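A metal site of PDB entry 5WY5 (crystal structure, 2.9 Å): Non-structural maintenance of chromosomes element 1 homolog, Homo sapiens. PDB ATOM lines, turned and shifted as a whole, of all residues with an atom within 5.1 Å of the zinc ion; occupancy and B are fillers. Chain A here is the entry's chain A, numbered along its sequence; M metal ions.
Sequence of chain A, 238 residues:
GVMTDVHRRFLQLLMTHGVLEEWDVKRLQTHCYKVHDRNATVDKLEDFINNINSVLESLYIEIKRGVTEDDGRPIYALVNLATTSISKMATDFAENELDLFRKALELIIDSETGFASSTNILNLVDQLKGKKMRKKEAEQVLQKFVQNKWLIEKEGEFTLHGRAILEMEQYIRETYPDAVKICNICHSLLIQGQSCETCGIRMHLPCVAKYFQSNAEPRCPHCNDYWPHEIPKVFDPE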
ATOM      1  N   CYS A 196      10.249  -6.912 -19.364  1.00  0.00           N
ATOM      2  CA  CYS A 196      11.204  -6.624 -18.292  1.00  0.00           C
ATOM      3  C   CYS A 196      12.077  -7.839 -18.080  1.00  0.00           C
ATOM      4  O   CYS A 196      11.613  -8.974 -18.234  1.00  0.00           O
ATOM      5  CB  CYS A 196      10.498  -6.218 -16.996  1.00  0.00           C
ATOM      6  SG  CYS A 196      11.644  -5.668 -15.662  1.00  0.00           S
ATOM      7  N   THR A 198      13.451  -8.649 -15.213  1.00  0.00           N
ATOM      8  CA  THR A 198      13.255  -9.191 -13.877  1.00  0.00           C
ATOM      9  C   THR A 198      11.859  -9.812 -13.753  1.00  0.00           C
ATOM     10  O   THR A 198      11.721 -10.973 -13.401  1.00  0.00           O
ATOM     11  CB  THR A 198      13.499  -8.117 -12.803  1.00  0.00           C
ATOM     12  OG1 THR A 198      14.687  -7.399 -13.133  1.00  0.00           O
ATOM     13  CG2 THR A 198      13.673  -8.773 -11.439  1.00  0.00           C
ATOM     14  N   CYS A 199      10.822  -9.035 -14.060  1.00  0.00           N
ATOM     15  CA  CYS A 199       9.520  -9.623 -14.243  1.00  0.00           C
ATOM     16  C   CYS A 199       9.627 -10.534 -15.426  1.00  0.00           C
ATOM     17  O   CYS A 199      10.672 -11.104 -15.718  1.00  0.00           O
ATOM     18  CB  CYS A 199       8.500  -8.546 -14.613  1.00  0.00           C
ATOM     19  SG  CYS A 199       7.977  -7.427 -13.314  1.00  0.00           S
ATOM     20  N   ILE A 201       7.214  -9.072 -17.458  1.00  0.00           N
ATOM     21  CA  ILE A 201       6.155  -8.158 -17.835  1.00  0.00           C
ATOM     22  C   ILE A 201       6.411  -7.582 -19.211  1.00  0.00           C
ATOM     23  O   ILE A 201       7.565  -7.388 -19.600  1.00  0.00           O
ATOM     24  CB  ILE A 201       5.935  -7.045 -16.785  1.00  0.00           C
ATOM     25  CG1 ILE A 201       4.632  -7.298 -16.035  1.00  0.00           C
ATOM     26  CG2 ILE A 201       5.836  -5.669 -17.423  1.00  0.00           C
ATOM     27  CD1 ILE A 201       4.630  -8.597 -15.244  1.00  0.00           C
ATOM     28  N   CYS A 220      10.230  -0.181 -13.940  1.00  0.00           N
ATOM     29  CA  CYS A 220       9.232  -1.210 -14.247  1.00  0.00           C
ATOM     30  C   CYS A 220       8.081  -1.167 -13.274  1.00  0.00           C
ATOM     31  O   CYS A 220       8.261  -1.376 -12.079  1.00  0.00           O
ATOM     32  CB  CYS A 220       9.892  -2.581 -14.191  1.00  0.00           C
ATOM     33  SG  CYS A 220       8.767  -3.965 -14.231  1.00  0.00           S
ATOM     34  N   HIS A 222       5.433  -3.049 -12.441  1.00  0.00           N
ATOM     35  CA  HIS A 222       5.356  -4.236 -11.594  1.00  0.00           C
ATOM     36  C   HIS A 222       6.795  -4.605 -11.274  1.00  0.00           C
ATOM     37  O   HIS A 222       7.554  -4.907 -12.178  1.00  0.00           O
ATOM     38  CB  HIS A 222       4.704  -5.377 -12.373  1.00  0.00           C
ATOM     39  CG  HIS A 222       4.416  -6.605 -11.543  1.00  0.00           C
ATOM     40  ND1 HIS A 222       3.290  -6.727 -10.759  1.00  0.00           N
ATOM     41  CD2 HIS A 222       5.106  -7.761 -11.398  1.00  0.00           C
ATOM     42  CE1 HIS A 222       3.295  -7.909 -10.169  1.00  0.00           C
ATOM     43  NE2 HIS A 222       4.384  -8.555 -10.533  1.00  0.00           N
ATOM     44  N   CYS A 223       7.175  -4.542  -9.996  1.00  0.00           N
ATOM     45  CA  CYS A 223       8.533  -4.894  -9.551  1.00  0.00           C
ATOM     46  C   CYS A 223       9.487  -3.720  -9.459  1.00  0.00           C
ATOM     47  O   CYS A 223      10.567  -3.820  -8.875  1.00  0.00           O
ATOM     48  CB  CYS A 223       9.174  -5.984 -10.417  1.00  0.00           C
ATOM     49  SG  CYS A 223      10.329  -5.362 -11.688  1.00  0.00           S
ATOM     50  N   ASP A 225      11.861  -2.427 -10.832  1.00  0.00           N
ATOM     51  CA  ASP A 225      13.259  -2.467 -11.253  1.00  0.00           C
ATOM     52  C   ASP A 225      13.480  -1.453 -12.363  1.00  0.00           C
ATOM     53  O   ASP A 225      12.543  -1.071 -13.068  1.00  0.00           O
ATOM     54  CB  ASP A 225      13.620  -3.876 -11.738  1.00  0.00           C
ATOM     55  CG  ASP A 225      15.095  -4.200 -11.550  1.00  0.00           C
ATOM     56  OD1 ASP A 225      15.796  -3.449 -10.832  1.00  0.00           O
ATOM     57  OD2 ASP A 225      15.556  -5.217 -12.114  1.00  0.00           O
HETATM   58 ZN    ZN M   1       9.747  -6.082 -14.009  1.00  0.00          ZN
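SG of Cys 199 lies close to O of His 222, 2.8 Å away. The backbone carbonyl oxygen of Ile 201 sits at hydrogen-bond distance from the backbone NH of Cys 196 (2.7 Å). The side-chain sulfur (SG) of Cys 196 lies close to the backbone NH (N) of Thr 198 (3.5 Å). The backbone NH (N) of Asp 225 lies close to the side-chain sulfur (SG) of Cys 223 (3.4 Å). The backbone NH of Cys 220 sits at hydrogen-bond distance from the backbone carbonyl oxygen of Asp 225 (2.6 Å). The side-chain sulfur (SG) of Cys 220 sits close to the backbone carbonyl oxygen (O) of His 222 (2.6 Å).
Merely in contact with the zinc ion: His 222. The nearest printed residue that does not touch the zinc ion is Thr 198 (4.3 Å).
SG of Cys 199 binds the zinc ion (2.3 Å). The side-chain sulfur (SG) of Cys 220 is bound to the zinc ion (2.3 Å). The zinc ion is bound by the side-chain sulfur (SG) of Cys 223 (2.5 Å). The zinc ion is bound by the side-chain sulfur (SG) of Cys 196 (2.5 Å).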
